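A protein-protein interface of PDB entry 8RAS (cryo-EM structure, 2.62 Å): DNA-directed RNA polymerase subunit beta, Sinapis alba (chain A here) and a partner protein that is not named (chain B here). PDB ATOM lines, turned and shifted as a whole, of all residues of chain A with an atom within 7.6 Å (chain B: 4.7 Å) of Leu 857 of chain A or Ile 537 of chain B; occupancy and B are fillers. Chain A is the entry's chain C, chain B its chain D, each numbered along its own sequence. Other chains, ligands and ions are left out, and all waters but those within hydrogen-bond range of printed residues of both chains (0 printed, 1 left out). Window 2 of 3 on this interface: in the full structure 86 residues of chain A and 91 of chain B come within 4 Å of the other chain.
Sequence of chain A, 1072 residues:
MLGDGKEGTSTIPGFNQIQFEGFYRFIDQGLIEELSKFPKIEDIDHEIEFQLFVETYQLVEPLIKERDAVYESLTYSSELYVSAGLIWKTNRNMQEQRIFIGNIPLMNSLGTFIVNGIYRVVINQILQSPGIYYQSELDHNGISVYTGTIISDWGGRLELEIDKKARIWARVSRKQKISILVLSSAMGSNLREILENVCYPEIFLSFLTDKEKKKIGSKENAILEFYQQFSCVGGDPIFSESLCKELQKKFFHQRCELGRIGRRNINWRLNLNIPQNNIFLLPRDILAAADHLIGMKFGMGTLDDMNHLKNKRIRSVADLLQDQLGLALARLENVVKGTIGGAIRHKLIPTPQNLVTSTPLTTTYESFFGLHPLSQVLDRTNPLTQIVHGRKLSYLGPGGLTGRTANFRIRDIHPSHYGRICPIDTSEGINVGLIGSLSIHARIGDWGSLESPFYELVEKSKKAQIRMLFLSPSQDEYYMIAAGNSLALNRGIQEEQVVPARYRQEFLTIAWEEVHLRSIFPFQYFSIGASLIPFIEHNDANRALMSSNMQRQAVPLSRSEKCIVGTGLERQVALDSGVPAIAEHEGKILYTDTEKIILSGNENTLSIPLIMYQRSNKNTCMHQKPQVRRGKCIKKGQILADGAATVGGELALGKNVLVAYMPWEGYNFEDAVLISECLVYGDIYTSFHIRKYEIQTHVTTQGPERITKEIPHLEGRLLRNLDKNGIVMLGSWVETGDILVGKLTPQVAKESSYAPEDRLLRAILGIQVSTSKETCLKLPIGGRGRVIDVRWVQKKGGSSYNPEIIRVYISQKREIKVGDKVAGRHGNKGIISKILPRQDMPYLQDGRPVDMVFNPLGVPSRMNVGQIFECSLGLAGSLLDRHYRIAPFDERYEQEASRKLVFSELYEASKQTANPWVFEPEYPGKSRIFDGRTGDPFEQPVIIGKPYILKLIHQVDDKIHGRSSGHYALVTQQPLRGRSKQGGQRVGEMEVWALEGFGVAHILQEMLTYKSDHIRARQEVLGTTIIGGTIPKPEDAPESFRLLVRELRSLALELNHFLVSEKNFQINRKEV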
ATOM      1  N   TYR A 661       5.746 -12.232 -16.733  1.00  0.00           N
ATOM      2  CA  TYR A 661       6.330 -13.058 -15.674  1.00  0.00           C
ATOM      3  C   TYR A 661       7.346 -12.212 -14.914  1.00  0.00           C
ATOM      4  O   TYR A 661       8.529 -12.193 -15.258  1.00  0.00           O
ATOM      5  CB  TYR A 661       6.986 -14.311 -16.241  1.00  0.00           C
ATOM      6  CG  TYR A 661       6.029 -15.421 -16.603  1.00  0.00           C
ATOM      7  CD1 TYR A 661       5.372 -15.425 -17.823  1.00  0.00           C
ATOM      8  CD2 TYR A 661       5.794 -16.472 -15.729  1.00  0.00           C
ATOM      9  CE1 TYR A 661       4.503 -16.436 -18.159  1.00  0.00           C
ATOM     10  CE2 TYR A 661       4.926 -17.491 -16.058  1.00  0.00           C
ATOM     11  CZ  TYR A 661       4.283 -17.466 -17.275  1.00  0.00           C
ATOM     12  OH  TYR A 661       3.415 -18.478 -17.611  1.00  0.00           O
ATOM     13  N   MET A 662       6.885 -11.519 -13.875  1.00  0.00           N
ATOM     14  CA  MET A 662       7.760 -10.677 -13.073  1.00  0.00           C
ATOM     15  C   MET A 662       7.142 -10.511 -11.696  1.00  0.00           C
ATOM     16  O   MET A 662       5.921 -10.638 -11.553  1.00  0.00           O
ATOM     17  CB  MET A 662       7.969  -9.308 -13.736  1.00  0.00           C
ATOM     18  CG  MET A 662       6.696  -8.683 -14.281  1.00  0.00           C
ATOM     19  SD  MET A 662       6.823  -6.900 -14.507  1.00  0.00           S
ATOM     20  CE  MET A 662       7.429  -6.397 -12.903  1.00  0.00           C
ATOM     21  N   PRO A 663       7.945 -10.251 -10.666  1.00  0.00           N
ATOM     22  CA  PRO A 663       7.376  -9.927  -9.354  1.00  0.00           C
ATOM     23  C   PRO A 663       6.825  -8.510  -9.336  1.00  0.00           C
ATOM     24  O   PRO A 663       7.424  -7.583  -9.885  1.00  0.00           O
ATOM     25  CB  PRO A 663       8.571 -10.071  -8.404  1.00  0.00           C
ATOM     26  CG  PRO A 663       9.755  -9.831  -9.255  1.00  0.00           C
ATOM     27  CD  PRO A 663       9.415 -10.336 -10.626  1.00  0.00           C
ATOM     28  N   ASN A 668       2.077 -11.069  -6.129  1.00  0.00           N
ATOM     29  CA  ASN A 668       2.194 -12.420  -6.661  1.00  0.00           C
ATOM     30  C   ASN A 668       3.163 -13.240  -5.817  1.00  0.00           C
ATOM     31  O   ASN A 668       3.889 -14.091  -6.334  1.00  0.00           O
ATOM     32  CB  ASN A 668       2.619 -12.406  -8.128  1.00  0.00           C
ATOM     33  CG  ASN A 668       3.757 -11.454  -8.400  1.00  0.00           C
ATOM     34  OD1 ASN A 668       4.408 -10.964  -7.480  1.00  0.00           O
ATOM     35  ND2 ASN A 668       4.007 -11.186  -9.674  1.00  0.00           N
ATOM     36  N   PHE A 669       3.180 -12.978  -4.512  1.00  0.00           N
ATOM     37  CA  PHE A 669       4.020 -13.731  -3.594  1.00  0.00           C
ATOM     38  C   PHE A 669       3.591 -15.192  -3.565  1.00  0.00           C
ATOM     39  O   PHE A 669       2.398 -15.506  -3.590  1.00  0.00           O
ATOM     40  CB  PHE A 669       3.936 -13.119  -2.195  1.00  0.00           C
ATOM     41  CG  PHE A 669       4.912 -13.698  -1.216  1.00  0.00           C
ATOM     42  CD1 PHE A 669       6.273 -13.617  -1.443  1.00  0.00           C
ATOM     43  CD2 PHE A 669       4.467 -14.303  -0.055  1.00  0.00           C
ATOM     44  CE1 PHE A 669       7.171 -14.144  -0.538  1.00  0.00           C
ATOM     45  CE2 PHE A 669       5.360 -14.831   0.852  1.00  0.00           C
ATOM     46  CZ  PHE A 669       6.713 -14.751   0.610  1.00  0.00           C
ATOM     47  N   GLU A 670       4.581 -16.085  -3.518  1.00  0.00           N
ATOM     48  CA  GLU A 670       4.359 -17.525  -3.581  1.00  0.00           C
ATOM     49  C   GLU A 670       3.609 -17.907  -4.851  1.00  0.00           C
ATOM     50  O   GLU A 670       4.221 -18.076  -5.911  1.00  0.00           O
ATOM     51  CB  GLU A 670       3.605 -18.021  -2.345  1.00  0.00           C
ATOM     52  CG  GLU A 670       4.243 -17.628  -1.025  1.00  0.00           C
ATOM     53  CD  GLU A 670       5.324 -18.594  -0.577  1.00  0.00           C
ATOM     54  OE1 GLU A 670       6.019 -19.165  -1.441  1.00  0.00           O
ATOM     55  OE2 GLU A 670       5.480 -18.780   0.648  1.00  0.00           O
ATOM     56  N   ASP A 671       2.285 -18.044  -4.759  1.00  0.00           N
ATOM     57  CA  ASP A 671       1.484 -18.487  -5.894  1.00  0.00           C
ATOM     58  C   ASP A 671       0.324 -17.544  -6.192  1.00  0.00           C
ATOM     59  O   ASP A 671      -0.626 -17.940  -6.870  1.00  0.00           O
ATOM     60  CB  ASP A 671       0.960 -19.903  -5.660  1.00  0.00           C
ATOM     61  CG  ASP A 671       1.793 -20.955  -6.361  1.00  0.00           C
ATOM     62  OD1 ASP A 671       2.959 -20.663  -6.697  1.00  0.00           O
ATOM     63  OD2 ASP A 671       1.281 -22.073  -6.575  1.00  0.00           O
ATOM     64  N   PHE A 854       2.588 -12.970 -13.486  1.00  0.00           N
ATOM     65  CA  PHE A 854       2.926 -14.209 -12.807  1.00  0.00           C
ATOM     66  C   PHE A 854       4.300 -14.097 -12.165  1.00  0.00           C
ATOM     67  O   PHE A 854       5.183 -13.395 -12.664  1.00  0.00           O
ATOM     68  CB  PHE A 854       2.907 -15.397 -13.775  1.00  0.00           C
ATOM     69  CG  PHE A 854       1.530 -15.836 -14.169  1.00  0.00           C
ATOM     70  CD1 PHE A 854       0.602 -16.195 -13.211  1.00  0.00           C
ATOM     71  CD2 PHE A 854       1.163 -15.893 -15.500  1.00  0.00           C
ATOM     72  CE1 PHE A 854      -0.666 -16.601 -13.575  1.00  0.00           C
ATOM     73  CE2 PHE A 854      -0.102 -16.297 -15.868  1.00  0.00           C
ATOM     74  CZ  PHE A 854      -1.017 -16.651 -14.905  1.00  0.00           C
ATOM     75  N   ASN A 855       4.469 -14.790 -11.051  1.00  0.00           N
ATOM     76  CA  ASN A 855       5.759 -14.807 -10.379  1.00  0.00           C
ATOM     77  C   ASN A 855       6.739 -15.667 -11.168  1.00  0.00           C
ATOM     78  O   ASN A 855       6.444 -16.834 -11.450  1.00  0.00           O
ATOM     79  CB  ASN A 855       5.612 -15.341  -8.957  1.00  0.00           C
ATOM     80  CG  ASN A 855       6.618 -14.737  -8.001  1.00  0.00           C
ATOM     81  OD1 ASN A 855       7.142 -13.650  -8.236  1.00  0.00           O
ATOM     82  ND2 ASN A 855       6.892 -15.441  -6.911  1.00  0.00           N
ATOM     83  N   PRO A 856       7.902 -15.135 -11.548  1.00  0.00           N
ATOM     84  CA  PRO A 856       8.888 -15.966 -12.253  1.00  0.00           C
ATOM     85  C   PRO A 856       9.547 -17.002 -11.364  1.00  0.00           C
ATOM     86  O   PRO A 856      10.149 -17.947 -11.887  1.00  0.00           O
ATOM     87  CB  PRO A 856       9.905 -14.939 -12.760  1.00  0.00           C
ATOM     88  CG  PRO A 856       9.844 -13.851 -11.754  1.00  0.00           C
ATOM     89  CD  PRO A 856       8.421 -13.790 -11.258  1.00  0.00           C
ATOM     90  N   LEU A 857       9.456 -16.854 -10.042  1.00  0.00           N
ATOM     91  CA  LEU A 857      10.054 -17.809  -9.119  1.00  0.00           C
ATOM     92  C   LEU A 857       9.353 -19.159  -9.128  1.00  0.00           C
ATOM     93  O   LEU A 857       9.917 -20.132  -8.617  1.00  0.00           O
ATOM     94  CB  LEU A 857      10.042 -17.238  -7.702  1.00  0.00           C
ATOM     95  CG  LEU A 857      11.230 -16.364  -7.302  1.00  0.00           C
ATOM     96  CD1 LEU A 857      11.071 -14.957  -7.853  1.00  0.00           C
ATOM     97  CD2 LEU A 857      11.372 -16.334  -5.793  1.00  0.00           C
ATOM     98  N   GLY A 858       8.149 -19.243  -9.691  1.00  0.00           N
ATOM     99  CA  GLY A 858       7.420 -20.494  -9.711  1.00  0.00           C
ATOM    100  C   GLY A 858       7.870 -21.490 -10.755  1.00  0.00           C
ATOM    101  O   GLY A 858       7.430 -22.640 -10.716  1.00  0.00           O
ATOM    102  N   VAL A 859       8.714 -21.079 -11.695  1.00  0.00           N
ATOM    103  CA  VAL A 859       9.208 -21.985 -12.730  1.00  0.00           C
ATOM    104  C   VAL A 859      10.345 -22.865 -12.213  1.00  0.00           C
ATOM    105  O   VAL A 859      10.258 -24.094 -12.346  1.00  0.00           O
ATOM    106  CB  VAL A 859       9.640 -21.211 -13.987  1.00  0.00           C
ATOM    107  CG1 VAL A 859       9.968 -22.176 -15.111  1.00  0.00           C
ATOM    108  CG2 VAL A 859       8.550 -20.243 -14.410  1.00  0.00           C
ATOM    109  N   PRO A 860      11.427 -22.314 -11.637  1.00  0.00           N
ATOM    110  CA  PRO A 860      12.571 -23.182 -11.298  1.00  0.00           C
ATOM    111  C   PRO A 860      12.252 -24.257 -10.277  1.00  0.00           C
ATOM    112  O   PRO A 860      12.694 -25.402 -10.435  1.00  0.00           O
ATOM    113  CB  PRO A 860      13.613 -22.189 -10.764  1.00  0.00           C
ATOM    114  CG  PRO A 860      13.203 -20.877 -11.304  1.00  0.00           C
ATOM    115  CD  PRO A 860      11.716 -20.912 -11.291  1.00  0.00           C
ATOM    116  N   SER A 861      11.505 -23.926  -9.224  1.00  0.00           N
ATOM    117  CA  SER A 861      11.176 -24.931  -8.220  1.00  0.00           C
ATOM    118  C   SER A 861      10.205 -25.966  -8.772  1.00  0.00           C
ATOM    119  O   SER A 861      10.304 -27.155  -8.449  1.00  0.00           O
ATOM    120  CB  SER A 861      10.598 -24.260  -6.974  1.00  0.00           C
ATOM    121  OG  SER A 861       9.598 -23.319  -7.321  1.00  0.00           O
ATOM    122  N   ARG A 862       9.259 -25.533  -9.607  1.00  0.00           N
ATOM    123  CA  ARG A 862       8.260 -26.439 -10.160  1.00  0.00           C
ATOM    124  C   ARG A 862       8.754 -27.161 -11.404  1.00  0.00           C
ATOM    125  O   ARG A 862       8.209 -28.216 -11.747  1.00  0.00           O
ATOM    126  CB  ARG A 862       6.976 -25.673 -10.486  1.00  0.00           C
ATOM    127  CG  ARG A 862       6.019 -25.469  -9.315  1.00  0.00           C
ATOM    128  CD  ARG A 862       6.708 -24.998  -8.041  1.00  0.00           C
ATOM    129  NE  ARG A 862       5.777 -24.829  -6.933  1.00  0.00           N
ATOM    130  CZ  ARG A 862       5.140 -23.700  -6.655  1.00  0.00           C
ATOM    131  NH1 ARG A 862       5.313 -22.612  -7.387  1.00  0.00           N
ATOM    132  NH2 ARG A 862       4.312 -23.662  -5.616  1.00  0.00           N
ATOM    133  N   MET A 863       9.758 -26.608 -12.087  1.00  0.00           N
ATOM    134  CA  MET A 863      10.421 -27.259 -13.217  1.00  0.00           C
ATOM    135  C   MET A 863       9.445 -27.587 -14.347  1.00  0.00           C
ATOM    136  O   MET A 863       9.408 -28.703 -14.865  1.00  0.00           O
ATOM    137  CB  MET A 863      11.172 -28.511 -12.755  1.00  0.00           C
ATOM    138  CG  MET A 863      12.498 -28.208 -12.071  1.00  0.00           C
ATOM    139  SD  MET A 863      13.193 -29.596 -11.157  1.00  0.00           S
ATOM    140  CE  MET A 863      11.736 -30.595 -10.886  1.00  0.00           C
ATOM    141  N   GLN B 533      12.237 -15.492  -0.640  1.00  0.00           N
ATOM    142  CA  GLN B 533      11.851 -15.459  -2.047  1.00  0.00           C
ATOM    143  C   GLN B 533      11.947 -14.065  -2.656  1.00  0.00           C
ATOM    144  O   GLN B 533      13.049 -13.584  -2.935  1.00  0.00           O
ATOM    145  CB  GLN B 533      10.437 -16.019  -2.210  1.00  0.00           C
ATOM    146  CG  GLN B 533      10.340 -17.492  -1.861  1.00  0.00           C
ATOM    147  CD  GLN B 533       8.927 -18.021  -1.928  1.00  0.00           C
ATOM    148  OE1 GLN B 533       8.137 -17.610  -2.776  1.00  0.00           O
ATOM    149  NE2 GLN B 533       8.600 -18.942  -1.030  1.00  0.00           N
ATOM    150  N   ASP B 534      10.801 -13.420  -2.879  1.00  0.00           N
ATOM    151  CA  ASP B 534      10.791 -12.137  -3.578  1.00  0.00           C
ATOM    152  C   ASP B 534      11.545 -11.069  -2.795  1.00  0.00           C
ATOM    153  O   ASP B 534      12.342 -10.315  -3.363  1.00  0.00           O
ATOM    154  CB  ASP B 534       9.352 -11.698  -3.842  1.00  0.00           C
ATOM    155  CG  ASP B 534       8.726 -12.429  -5.007  1.00  0.00           C
ATOM    156  OD1 ASP B 534       9.478 -12.882  -5.893  1.00  0.00           O
ATOM    157  OD2 ASP B 534       7.484 -12.550  -5.040  1.00  0.00           O
ATOM    158  N   MET B 535      11.302 -10.985  -1.484  1.00  0.00           N
ATOM    159  CA  MET B 535      12.034 -10.022  -0.668  1.00  0.00           C
ATOM    160  C   MET B 535      13.521 -10.343  -0.652  1.00  0.00           C
ATOM    161  O   MET B 535      14.363  -9.438  -0.695  1.00  0.00           O
ATOM    162  CB  MET B 535      11.480  -9.997   0.756  1.00  0.00           C
ATOM    163  CG  MET B 535       9.972 -10.102   0.855  1.00  0.00           C
ATOM    164  SD  MET B 535       9.438 -10.609   2.500  1.00  0.00           S
ATOM    165  CE  MET B 535       8.273 -11.903   2.098  1.00  0.00           C
ATOM    166  N   LEU B 536      13.862 -11.631  -0.586  1.00  0.00           N
ATOM    167  CA  LEU B 536      15.264 -12.029  -0.592  1.00  0.00           C
ATOM    168  C   LEU B 536      15.942 -11.648  -1.902  1.00  0.00           C
ATOM    169  O   LEU B 536      17.075 -11.155  -1.898  1.00  0.00           O
ATOM    170  CB  LEU B 536      15.377 -13.531  -0.340  1.00  0.00           C
ATOM    171  CG  LEU B 536      16.665 -14.015   0.319  1.00  0.00           C
ATOM    172  CD1 LEU B 536      17.065 -13.076   1.439  1.00  0.00           C
ATOM    173  CD2 LEU B 536      16.482 -15.426   0.840  1.00  0.00           C
ATOM    174  N   ILE B 537      15.268 -11.869  -3.034  1.00  0.00           N
ATOM    175  CA  ILE B 537      15.831 -11.483  -4.326  1.00  0.00           C
ATOM    176  C   ILE B 537      15.982  -9.971  -4.413  1.00  0.00           C
ATOM    177  O   ILE B 537      16.984  -9.461  -4.928  1.00  0.00           O
ATOM    178  CB  ILE B 537      14.970 -12.038  -5.479  1.00  0.00           C
ATOM    179  CG1 ILE B 537      15.418 -13.451  -5.846  1.00  0.00           C
ATOM    180  CG2 ILE B 537      15.039 -11.137  -6.701  1.00  0.00           C
ATOM    181  CD1 ILE B 537      14.322 -14.297  -6.432  1.00  0.00           C
ATOM    182  N   GLY B 538      14.988  -9.231  -3.919  1.00  0.00           N
ATOM    183  CA  GLY B 538      15.092  -7.780  -3.930  1.00  0.00           C
ATOM    184  C   GLY B 538      16.278  -7.279  -3.130  1.00  0.00           C
ATOM    185  O   GLY B 538      17.035  -6.421  -3.589  1.00  0.00           O
ATOM    186  N   LEU B 539      16.464  -7.823  -1.925  1.00  0.00           N
ATOM    187  CA  LEU B 539      17.604  -7.427  -1.103  1.00  0.00           C
ATOM    188  C   LEU B 539      18.924  -7.840  -1.740  1.00  0.00           C
ATOM    189  O   LEU B 539      19.906  -7.092  -1.687  1.00  0.00           O
ATOM    190  CB  LEU B 539      17.477  -8.025   0.296  1.00  0.00           C
ATOM    191  CG  LEU B 539      16.277  -7.571   1.125  1.00  0.00           C
ATOM    192  CD1 LEU B 539      16.270  -8.280   2.464  1.00  0.00           C
ATOM    193  CD2 LEU B 539      16.285  -6.065   1.306  1.00  0.00           C
ATOM    194  N   TYR B 540      18.970  -9.033  -2.339  1.00  0.00           N
ATOM    195  CA  TYR B 540      20.191  -9.499  -2.985  1.00  0.00           C
ATOM    196  C   TYR B 540      20.575  -8.602  -4.152  1.00  0.00           C
ATOM    197  O   TYR B 540      21.753  -8.277  -4.334  1.00  0.00           O
ATOM    198  CB  TYR B 540      20.008 -10.942  -3.454  1.00  0.00           C
ATOM    199  CG  TYR B 540      21.245 -11.565  -4.057  1.00  0.00           C
ATOM    200  CD1 TYR B 540      22.198 -12.174  -3.256  1.00  0.00           C
ATOM    201  CD2 TYR B 540      21.453 -11.555  -5.429  1.00  0.00           C
ATOM    202  CE1 TYR B 540      23.325 -12.748  -3.801  1.00  0.00           C
ATOM    203  CE2 TYR B 540      22.578 -12.125  -5.982  1.00  0.00           C
ATOM    204  CZ  TYR B 540      23.511 -12.721  -5.164  1.00  0.00           C
ATOM    205  OH  TYR B 540      24.634 -13.292  -5.711  1.00  0.00           O
ATOM    206  N   VAL B 541      19.592  -8.197  -4.958  1.00  0.00           N
ATOM    207  CA  VAL B 541      19.872  -7.307  -6.078  1.00  0.00           C
ATOM    208  C   VAL B 541      20.268  -5.925  -5.575  1.00  0.00           C
ATOM    209  O   VAL B 541      21.172  -5.285  -6.123  1.00  0.00           O
ATOM    210  CB  VAL B 541      18.658  -7.247  -7.022  1.00  0.00           C
ATOM    211  CG1 VAL B 541      18.794  -6.093  -7.994  1.00  0.00           C
ATOM    212  CG2 VAL B 541      18.510  -8.560  -7.770  1.00  0.00           C
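The backbone carbonyl oxygen of Asn 668 of chain A sits close to the side-chain amide nitrogen of Asn 855 of chain A, at 3.3 Å. The side-chain hydroxyl (OG) of Ser 861 of chain A sits at hydrogen-bond distance from the backbone carbonyl oxygen (O) of Leu 857 of chain A (3.5 Å).
OD1 of Asp 534 of chain B touches CB of Pro 663 of chain A, 3.9 Å away. OD2 of Asp 534 of chain B touches CA of Phe 669 of chain A (3.9 Å). Phe 669 of chain A touches Met 535 of chain B (CZ to CE, 3.6 Å). CB of Gln 533 of chain B touches CD2 of Leu 857 of chain A, 3.7 Å away. Asp 534 of chain B touches Leu 857 of chain A. Leu 857 of chain A touches Ile 537 of chain B.
Of the 17 printed residues of chain A, 5 touch a printed residue of chain B. Printed residues of chain A that touch a printed residue of chain B: Pro 663, Phe 669, Glu 670, Asn 855 and Leu 857. Of the 9 printed residues of chain B, 4 touch a printed residue of chain A. Hydrophobic or aromatic side chains of chain B that line the printed part of chain A: Met 535 and Ile 537. Among the printed residues, 8 pairs touch across the chains.
Leu 857 of chain A touches three residues of chain B. Ile 537 of chain B touches just one residue of chain A: Leu 857 (3.6 Å). Of the printed residues of chain A, Met 535 of chain B touches Phe 669 (3.6 Å). Of the printed residues of chain A, Gln 533 of chain B touches Glu 670 and Leu 857. Of the printed residues of chain B, Glu 670 of chain A touches Gln 533 (2.6 Å). Of the printed residues of chain B, Asn 855 of chain A touches Asp 534 (3.4 Å). Leu 539 of chain B touches none of the printed residues of chain A. Val 859 of chain A touches none of the printed residues of chain B.
The side-chain carboxylate (OE1) of Glu 670 of chain A lies within hydrogen-bond range of the side-chain amide nitrogen (NE2) of Gln 533 of chain B, 2.6 Å away. OD1 of Asn 855 of chain A sits close to OD1 of Asp 534 of chain B (3.4 Å).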
